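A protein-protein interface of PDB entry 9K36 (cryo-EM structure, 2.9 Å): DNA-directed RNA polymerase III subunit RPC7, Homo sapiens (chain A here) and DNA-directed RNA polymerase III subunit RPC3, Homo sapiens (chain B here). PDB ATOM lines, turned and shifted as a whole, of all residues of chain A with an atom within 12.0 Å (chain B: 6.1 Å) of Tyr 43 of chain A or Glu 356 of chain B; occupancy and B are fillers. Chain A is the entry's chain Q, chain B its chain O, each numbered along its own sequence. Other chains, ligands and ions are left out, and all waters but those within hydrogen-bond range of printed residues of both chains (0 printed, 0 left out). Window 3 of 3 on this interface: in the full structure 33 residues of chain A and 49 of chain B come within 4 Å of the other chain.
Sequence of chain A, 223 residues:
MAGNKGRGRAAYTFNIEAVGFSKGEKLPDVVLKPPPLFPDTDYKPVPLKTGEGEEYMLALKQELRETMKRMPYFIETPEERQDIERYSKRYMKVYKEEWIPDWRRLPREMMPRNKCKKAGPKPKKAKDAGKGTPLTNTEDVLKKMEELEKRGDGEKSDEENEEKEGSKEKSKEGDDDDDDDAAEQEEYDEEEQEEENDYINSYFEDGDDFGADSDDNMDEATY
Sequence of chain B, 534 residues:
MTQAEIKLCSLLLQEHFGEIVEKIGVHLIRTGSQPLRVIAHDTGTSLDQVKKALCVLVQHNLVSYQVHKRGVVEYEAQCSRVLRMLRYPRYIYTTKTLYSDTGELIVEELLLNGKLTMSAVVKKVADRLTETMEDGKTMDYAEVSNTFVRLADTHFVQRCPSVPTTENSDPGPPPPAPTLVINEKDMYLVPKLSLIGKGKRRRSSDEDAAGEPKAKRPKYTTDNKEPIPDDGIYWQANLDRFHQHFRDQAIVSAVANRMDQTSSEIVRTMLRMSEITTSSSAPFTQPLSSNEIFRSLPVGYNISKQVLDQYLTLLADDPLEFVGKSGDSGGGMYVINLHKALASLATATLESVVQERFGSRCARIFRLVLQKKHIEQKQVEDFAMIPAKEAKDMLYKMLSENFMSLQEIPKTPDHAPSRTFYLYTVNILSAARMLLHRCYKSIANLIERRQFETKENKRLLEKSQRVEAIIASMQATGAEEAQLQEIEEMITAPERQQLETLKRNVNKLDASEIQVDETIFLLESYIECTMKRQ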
ATOM      1  N   PHE A  38     -12.550  -5.259  -7.273  1.00  0.00           N
ATOM      2  CA  PHE A  38     -12.653  -5.499  -8.711  1.00  0.00           C
ATOM      3  C   PHE A  38     -13.064  -4.196  -9.384  1.00  0.00           C
ATOM      4  O   PHE A  38     -14.263  -3.894  -9.497  1.00  0.00           O
ATOM      5  CB  PHE A  38     -13.649  -6.617  -9.015  1.00  0.00           C
ATOM      6  CG  PHE A  38     -13.255  -7.948  -8.439  1.00  0.00           C
ATOM      7  CD1 PHE A  38     -13.654  -8.311  -7.160  1.00  0.00           C
ATOM      8  CD2 PHE A  38     -12.486  -8.836  -9.172  1.00  0.00           C
ATOM      9  CE1 PHE A  38     -13.291  -9.534  -6.629  1.00  0.00           C
ATOM     10  CE2 PHE A  38     -12.121 -10.058  -8.646  1.00  0.00           C
ATOM     11  CZ  PHE A  38     -12.524 -10.407  -7.373  1.00  0.00           C
ATOM     12  N   PRO A  39     -12.105  -3.390  -9.840  1.00  0.00           N
ATOM     13  CA  PRO A  39     -12.461  -2.123 -10.494  1.00  0.00           C
ATOM     14  C   PRO A  39     -13.152  -2.361 -11.828  1.00  0.00           C
ATOM     15  O   PRO A  39     -12.815  -3.286 -12.569  1.00  0.00           O
ATOM     16  CB  PRO A  39     -11.107  -1.426 -10.672  1.00  0.00           C
ATOM     17  CG  PRO A  39     -10.116  -2.542 -10.704  1.00  0.00           C
ATOM     18  CD  PRO A  39     -10.649  -3.582  -9.759  1.00  0.00           C
ATOM     19  N   ASP A  40     -14.125  -1.507 -12.131  1.00  0.00           N
ATOM     20  CA  ASP A  40     -14.892  -1.655 -13.360  1.00  0.00           C
ATOM     21  C   ASP A  40     -14.073  -1.221 -14.571  1.00  0.00           C
ATOM     22  O   ASP A  40     -13.193  -0.360 -14.482  1.00  0.00           O
ATOM     23  CB  ASP A  40     -16.184  -0.839 -13.285  1.00  0.00           C
ATOM     24  CG  ASP A  40     -15.941   0.603 -12.881  1.00  0.00           C
ATOM     25  OD1 ASP A  40     -14.806   0.926 -12.476  1.00  0.00           O
ATOM     26  OD2 ASP A  40     -16.887   1.414 -12.970  1.00  0.00           O
ATOM     27  N   THR A  41     -14.373  -1.833 -15.715  1.00  0.00           N
ATOM     28  CA  THR A  41     -13.705  -1.532 -16.973  1.00  0.00           C
ATOM     29  C   THR A  41     -14.748  -1.254 -18.045  1.00  0.00           C
ATOM     30  O   THR A  41     -15.777  -1.934 -18.115  1.00  0.00           O
ATOM     31  CB  THR A  41     -12.797  -2.684 -17.421  1.00  0.00           C
ATOM     32  OG1 THR A  41     -13.564  -3.890 -17.518  1.00  0.00           O
ATOM     33  CG2 THR A  41     -11.662  -2.888 -16.430  1.00  0.00           C
ATOM     34  N   ASP A  42     -14.475  -0.251 -18.877  1.00  0.00           N
ATOM     35  CA  ASP A  42     -15.381   0.120 -19.957  1.00  0.00           C
ATOM     36  C   ASP A  42     -15.242  -0.767 -21.186  1.00  0.00           C
ATOM     37  O   ASP A  42     -16.065  -0.663 -22.101  1.00  0.00           O
ATOM     38  CB  ASP A  42     -15.155   1.584 -20.348  1.00  0.00           C
ATOM     39  CG  ASP A  42     -13.690   1.906 -20.571  1.00  0.00           C
ATOM     40  OD1 ASP A  42     -12.839   1.055 -20.249  1.00  0.00           O
ATOM     41  OD2 ASP A  42     -13.394   3.011 -21.072  1.00  0.00           O
ATOM     42  N   TYR A  43     -14.228  -1.628 -21.235  1.00  0.00           N
ATOM     43  CA  TYR A  43     -14.032  -2.559 -22.339  1.00  0.00           C
ATOM     44  C   TYR A  43     -14.434  -3.957 -21.896  1.00  0.00           C
ATOM     45  O   TYR A  43     -13.983  -4.437 -20.852  1.00  0.00           O
ATOM     46  CB  TYR A  43     -12.578  -2.548 -22.815  1.00  0.00           C
ATOM     47  CG  TYR A  43     -12.129  -1.221 -23.385  1.00  0.00           C
ATOM     48  CD1 TYR A  43     -12.458  -0.855 -24.682  1.00  0.00           C
ATOM     49  CD2 TYR A  43     -11.373  -0.339 -22.626  1.00  0.00           C
ATOM     50  CE1 TYR A  43     -12.051   0.358 -25.207  1.00  0.00           C
ATOM     51  CE2 TYR A  43     -10.962   0.877 -23.142  1.00  0.00           C
ATOM     52  CZ  TYR A  43     -11.301   1.218 -24.433  1.00  0.00           C
ATOM     53  OH  TYR A  43     -10.893   2.427 -24.952  1.00  0.00           O
ATOM     54  N   LYS A  44     -15.279  -4.602 -22.688  1.00  0.00           N
ATOM     55  CA  LYS A  44     -15.779  -5.934 -22.396  1.00  0.00           C
ATOM     56  C   LYS A  44     -15.145  -6.961 -23.322  1.00  0.00           C
ATOM     57  O   LYS A  44     -14.712  -6.632 -24.434  1.00  0.00           O
ATOM     58  CB  LYS A  44     -17.307  -5.980 -22.543  1.00  0.00           C
ATOM     59  CG  LYS A  44     -18.041  -4.933 -21.718  1.00  0.00           C
ATOM     60  CD  LYS A  44     -17.700  -5.048 -20.239  1.00  0.00           C
ATOM     61  CE  LYS A  44     -18.173  -6.372 -19.657  1.00  0.00           C
ATOM     62  NZ  LYS A  44     -17.825  -6.501 -18.217  1.00  0.00           N
ATOM     63  N   PRO A  45     -15.052  -8.219 -22.892  1.00  0.00           N
ATOM     64  CA  PRO A  45     -14.457  -9.250 -23.752  1.00  0.00           C
ATOM     65  C   PRO A  45     -15.247  -9.431 -25.039  1.00  0.00           C
ATOM     66  O   PRO A  45     -16.478  -9.347 -25.058  1.00  0.00           O
ATOM     67  CB  PRO A  45     -14.507 -10.511 -22.881  1.00  0.00           C
ATOM     68  CG  PRO A  45     -14.544 -10.000 -21.480  1.00  0.00           C
ATOM     69  CD  PRO A  45     -15.343  -8.730 -21.540  1.00  0.00           C
ATOM     70  N   VAL A  46     -14.518  -9.674 -26.127  1.00  0.00           N
ATOM     71  CA  VAL A  46     -15.157  -9.900 -27.426  1.00  0.00           C
ATOM     72  C   VAL A  46     -15.964 -11.191 -27.366  1.00  0.00           C
ATOM     73  O   VAL A  46     -15.490 -12.187 -26.784  1.00  0.00           O
ATOM     74  CB  VAL A  46     -14.096  -9.962 -28.540  1.00  0.00           C
ATOM     75  CG1 VAL A  46     -14.737 -10.239 -29.892  1.00  0.00           C
ATOM     76  CG2 VAL A  46     -13.299  -8.665 -28.582  1.00  0.00           C
ATOM     77  N   PRO A  47     -17.181 -11.233 -27.912  1.00  0.00           N
ATOM     78  CA  PRO A  47     -17.937 -12.489 -27.917  1.00  0.00           C
ATOM     79  C   PRO A  47     -17.197 -13.585 -28.674  1.00  0.00           C
ATOM     80  O   PRO A  47     -16.462 -13.326 -29.629  1.00  0.00           O
ATOM     81  CB  PRO A  47     -19.250 -12.113 -28.619  1.00  0.00           C
ATOM     82  CG  PRO A  47     -18.960 -10.831 -29.336  1.00  0.00           C
ATOM     83  CD  PRO A  47     -17.956 -10.121 -28.484  1.00  0.00           C
ATOM     84  N   LEU A  48     -17.395 -14.820 -28.222  1.00  0.00           N
ATOM     85  CA  LEU A  48     -16.692 -15.958 -28.793  1.00  0.00           C
ATOM     86  C   LEU A  48     -17.123 -16.200 -30.235  1.00  0.00           C
ATOM     87  O   LEU A  48     -18.234 -15.853 -30.645  1.00  0.00           O
ATOM     88  CB  LEU A  48     -16.937 -17.217 -27.960  1.00  0.00           C
ATOM     89  CG  LEU A  48     -16.217 -17.360 -26.615  1.00  0.00           C
ATOM     90  CD1 LEU A  48     -14.735 -17.051 -26.764  1.00  0.00           C
ATOM     91  CD2 LEU A  48     -16.851 -16.493 -25.531  1.00  0.00           C
ATOM     92  N   LYS A  49     -16.222 -16.803 -31.007  1.00  0.00           N
ATOM     93  CA  LYS A  49     -16.524 -17.144 -32.390  1.00  0.00           C
ATOM     94  C   LYS A  49     -17.618 -18.203 -32.446  1.00  0.00           C
ATOM     95  O   LYS A  49     -17.677 -19.105 -31.607  1.00  0.00           O
ATOM     96  CB  LYS A  49     -15.267 -17.645 -33.100  1.00  0.00           C
ATOM     97  CG  LYS A  49     -14.103 -16.666 -33.072  1.00  0.00           C
ATOM     98  CD  LYS A  49     -12.866 -17.259 -33.726  1.00  0.00           C
ATOM     99  CE  LYS A  49     -13.113 -17.584 -35.191  1.00  0.00           C
ATOM    100  NZ  LYS A  49     -13.464 -16.372 -35.980  1.00  0.00           N
ATOM    101  N   GLU B 351      -1.201  -6.390 -31.463  1.00  0.00           N
ATOM    102  CA  GLU B 351      -1.952  -5.158 -31.668  1.00  0.00           C
ATOM    103  C   GLU B 351      -3.440  -5.377 -31.417  1.00  0.00           C
ATOM    104  O   GLU B 351      -4.123  -4.488 -30.895  1.00  0.00           O
ATOM    105  CB  GLU B 351      -1.706  -4.603 -33.074  1.00  0.00           C
ATOM    106  CG  GLU B 351      -2.294  -5.423 -34.207  1.00  0.00           C
ATOM    107  CD  GLU B 351      -2.003  -4.826 -35.570  1.00  0.00           C
ATOM    108  OE1 GLU B 351      -1.220  -3.856 -35.640  1.00  0.00           O
ATOM    109  OE2 GLU B 351      -2.557  -5.327 -36.572  1.00  0.00           O
ATOM    110  N   SER B 352      -3.952  -6.569 -31.735  1.00  0.00           N
ATOM    111  CA  SER B 352      -5.359  -6.857 -31.481  1.00  0.00           C
ATOM    112  C   SER B 352      -5.652  -6.927 -29.989  1.00  0.00           C
ATOM    113  O   SER B 352      -6.666  -6.391 -29.524  1.00  0.00           O
ATOM    114  CB  SER B 352      -5.758  -8.161 -32.169  1.00  0.00           C
ATOM    115  OG  SER B 352      -7.122  -8.467 -31.928  1.00  0.00           O
ATOM    116  N   VAL B 353      -4.778  -7.579 -29.216  1.00  0.00           N
ATOM    117  CA  VAL B 353      -5.019  -7.668 -27.780  1.00  0.00           C
ATOM    118  C   VAL B 353      -4.858  -6.300 -27.127  1.00  0.00           C
ATOM    119  O   VAL B 353      -5.602  -5.949 -26.202  1.00  0.00           O
ATOM    120  CB  VAL B 353      -4.120  -8.740 -27.127  1.00  0.00           C
ATOM    121  CG1 VAL B 353      -2.654  -8.365 -27.204  1.00  0.00           C
ATOM    122  CG2 VAL B 353      -4.534  -8.971 -25.680  1.00  0.00           C
ATOM    123  N   VAL B 354      -3.920  -5.482 -27.622  1.00  0.00           N
ATOM    124  CA  VAL B 354      -3.784  -4.122 -27.106  1.00  0.00           C
ATOM    125  C   VAL B 354      -5.042  -3.310 -27.402  1.00  0.00           C
ATOM    126  O   VAL B 354      -5.545  -2.585 -26.535  1.00  0.00           O
ATOM    127  CB  VAL B 354      -2.524  -3.453 -27.689  1.00  0.00           C
ATOM    128  CG1 VAL B 354      -2.547  -1.953 -27.431  1.00  0.00           C
ATOM    129  CG2 VAL B 354      -1.274  -4.073 -27.085  1.00  0.00           C
ATOM    130  N   GLN B 355      -5.570  -3.426 -28.624  1.00  0.00           N
ATOM    131  CA  GLN B 355      -6.777  -2.692 -28.986  1.00  0.00           C
ATOM    132  C   GLN B 355      -7.966  -3.126 -28.138  1.00  0.00           C
ATOM    133  O   GLN B 355      -8.752  -2.288 -27.681  1.00  0.00           O
ATOM    134  CB  GLN B 355      -7.082  -2.886 -30.471  1.00  0.00           C
ATOM    135  CG  GLN B 355      -8.296  -2.114 -30.963  1.00  0.00           C
ATOM    136  CD  GLN B 355      -8.540  -2.294 -32.448  1.00  0.00           C
ATOM    137  OE1 GLN B 355      -7.754  -2.931 -33.146  1.00  0.00           O
ATOM    138  NE2 GLN B 355      -9.639  -1.731 -32.939  1.00  0.00           N
ATOM    139  N   GLU B 356      -8.117  -4.433 -27.918  1.00  0.00           N
ATOM    140  CA  GLU B 356      -9.257  -4.922 -27.155  1.00  0.00           C
ATOM    141  C   GLU B 356      -9.094  -4.711 -25.655  1.00  0.00           C
ATOM    142  O   GLU B 356     -10.093  -4.770 -24.927  1.00  0.00           O
ATOM    143  CB  GLU B 356      -9.493  -6.404 -27.453  1.00  0.00           C
ATOM    144  CG  GLU B 356      -9.961  -6.688 -28.873  1.00  0.00           C
ATOM    145  CD  GLU B 356     -11.356  -6.155 -29.153  1.00  0.00           C
ATOM    146  OE1 GLU B 356     -12.119  -5.939 -28.188  1.00  0.00           O
ATOM    147  OE2 GLU B 356     -11.688  -5.951 -30.337  1.00  0.00           O
ATOM    148  N   ARG B 357      -7.877  -4.468 -25.172  1.00  0.00           N
ATOM    149  CA  ARG B 357      -7.685  -4.242 -23.746  1.00  0.00           C
ATOM    150  C   ARG B 357      -7.677  -2.767 -23.367  1.00  0.00           C
ATOM    151  O   ARG B 357      -8.104  -2.422 -22.260  1.00  0.00           O
ATOM    152  CB  ARG B 357      -6.382  -4.900 -23.279  1.00  0.00           C
ATOM    153  CG  ARG B 357      -6.192  -4.898 -21.772  1.00  0.00           C
ATOM    154  CD  ARG B 357      -4.919  -5.622 -21.365  1.00  0.00           C
ATOM    155  NE  ARG B 357      -4.708  -5.574 -19.922  1.00  0.00           N
ATOM    156  CZ  ARG B 357      -3.649  -6.087 -19.305  1.00  0.00           C
ATOM    157  NH1 ARG B 357      -2.697  -6.687 -20.005  1.00  0.00           N
ATOM    158  NH2 ARG B 357      -3.539  -5.998 -17.986  1.00  0.00           N
ATOM    159  N   PHE B 358      -7.213  -1.883 -24.253  1.00  0.00           N
ATOM    160  CA  PHE B 358      -7.096  -0.471 -23.912  1.00  0.00           C
ATOM    161  C   PHE B 358      -7.754   0.474 -24.910  1.00  0.00           C
ATOM    162  O   PHE B 358      -7.656   1.694 -24.728  1.00  0.00           O
ATOM    163  CB  PHE B 358      -5.619  -0.080 -23.755  1.00  0.00           C
ATOM    164  CG  PHE B 358      -4.893  -0.858 -22.697  1.00  0.00           C
ATOM    165  CD1 PHE B 358      -5.094  -0.582 -21.355  1.00  0.00           C
ATOM    166  CD2 PHE B 358      -4.004  -1.860 -23.046  1.00  0.00           C
ATOM    167  CE1 PHE B 358      -4.426  -1.295 -20.378  1.00  0.00           C
ATOM    168  CE2 PHE B 358      -3.330  -2.575 -22.073  1.00  0.00           C
ATOM    169  CZ  PHE B 358      -3.543  -2.291 -20.739  1.00  0.00           C
ATOM    170  N   GLY B 359      -8.409  -0.034 -25.947  1.00  0.00           N
ATOM    171  CA  GLY B 359      -9.109   0.808 -26.894  1.00  0.00           C
ATOM    172  C   GLY B 359      -8.337   1.007 -28.188  1.00  0.00           C
ATOM    173  O   GLY B 359      -7.215   0.525 -28.371  1.00  0.00           O
ATOM    174  N   SER B 360      -8.970   1.742 -29.106  1.00  0.00           N
ATOM    175  CA  SER B 360      -8.388   1.953 -30.428  1.00  0.00           C
ATOM    176  C   SER B 360      -7.275   2.992 -30.406  1.00  0.00           C
ATOM    177  O   SER B 360      -6.321   2.887 -31.183  1.00  0.00           O
ATOM    178  CB  SER B 360      -9.477   2.366 -31.420  1.00  0.00           C
ATOM    179  OG  SER B 360     -10.474   1.367 -31.532  1.00  0.00           O
ATOM    180  N   ARG B 361      -7.378   4.001 -29.534  1.00  0.00           N
ATOM    181  CA  ARG B 361      -6.338   5.024 -29.470  1.00  0.00           C
ATOM    182  C   ARG B 361      -5.034   4.453 -28.926  1.00  0.00           C
ATOM    183  O   ARG B 361      -3.945   4.787 -29.414  1.00  0.00           O
ATOM    184  CB  ARG B 361      -6.814   6.199 -28.618  1.00  0.00           C
ATOM    185  CG  ARG B 361      -8.170   6.747 -29.031  1.00  0.00           C
ATOM    186  CD  ARG B 361      -8.620   7.875 -28.117  1.00  0.00           C
ATOM    187  NE  ARG B 361      -7.769   9.055 -28.241  1.00  0.00           N
ATOM    188  CZ  ARG B 361      -7.992  10.051 -29.091  1.00  0.00           C
ATOM    189  NH1 ARG B 361      -9.040  10.011 -29.901  1.00  0.00           N
ATOM    190  NH2 ARG B 361      -7.165  11.087 -29.133  1.00  0.00           N
ATOM    191  N   MET B 394      -1.844   6.417 -21.477  1.00  0.00           N
ATOM    192  CA  MET B 394      -1.847   5.106 -22.118  1.00  0.00           C
ATOM    193  C   MET B 394      -0.433   4.545 -22.236  1.00  0.00           C
ATOM    194  O   MET B 394      -0.228   3.332 -22.106  1.00  0.00           O
ATOM    195  CB  MET B 394      -2.511   5.195 -23.491  1.00  0.00           C
ATOM    196  CG  MET B 394      -3.974   5.606 -23.446  1.00  0.00           C
ATOM    197  SD  MET B 394      -4.731   5.703 -25.082  1.00  0.00           S
ATOM    198  CE  MET B 394      -6.405   6.172 -24.654  1.00  0.00           C
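Tyr 43 of chain A touches just these residues of chain B: Glu 356, Arg 357, Phe 358 and Gly 359.
Of chain A, only Tyr 43 (3.9 Å) and Val 46 (3.0 Å) come within 4 Å of Glu 356 of chain B.
No residue of chain A comes within 4 Å of Val 353 of chain B.
Val 354 of chain B touches none of the printed residues of chain A.
Gly 359 of chain B touches just one residue of chain A: Tyr 43 (3.1 Å).
No residue of chain A comes within 4 Å of Ser 360 of chain B.
Printed residues of chain B within 4 Å of Val 46 of chain A: Glu 356 (3.0 Å).
Printed residues of chain A within 4 Å of Arg 357 of chain B: Tyr 43 (3.9 Å).
The nearest residue of chain B that does not touch Tyr 43 of chain A is Ser 360 of chain B (4.6 Å).
The nearest residue of chain A that does not touch Glu 356 of chain B is Lys 44 of chain A (4.6 Å).
The nearest printed residue of chain A that does not touch Arg 357 of chain B is Asp 42 of chain A (6.2 Å).
Of the 12 printed residues of chain B, 4 touch a printed residue of chain A.
Printed residues of chain B that touch a printed residue of chain A: Glu 356, Arg 357, Phe 358 and Gly 359.
Of the 12 printed residues of chain A, 2 touch a printed residue of chain B.
Hydrophobic or aromatic side chains of chain A that line the printed part of chain B: Tyr 43 and Val 46.
Among the printed residues, 5 pairs touch across the chains.
Among the printed residues, no Asp or Glu carboxylate lies within 4 Å of a Lys or Arg side-chain nitrogen of the other chain.
Glu 356 of chain B touches Tyr 43 of chain A (O to CB, 3.9 Å).
Arg 357 of chain B touches Tyr 43 of chain A (O to CD2, 3.9 Å).
OH of Tyr 43 of chain A touches CA of Gly 359 of chain B (3.1 Å).
Val 46 of chain A touches Glu 356 of chain B.
O of Phe 358 of chain B sits at hydrogen-bond distance from OH of Tyr 43 of chain A.
The backbone carbonyl oxygen (O) of Tyr 43 of chain A lies within hydrogen-bond range of the side-chain hydroxyl (OG1) of Thr 41 of chain A (3.4 Å).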
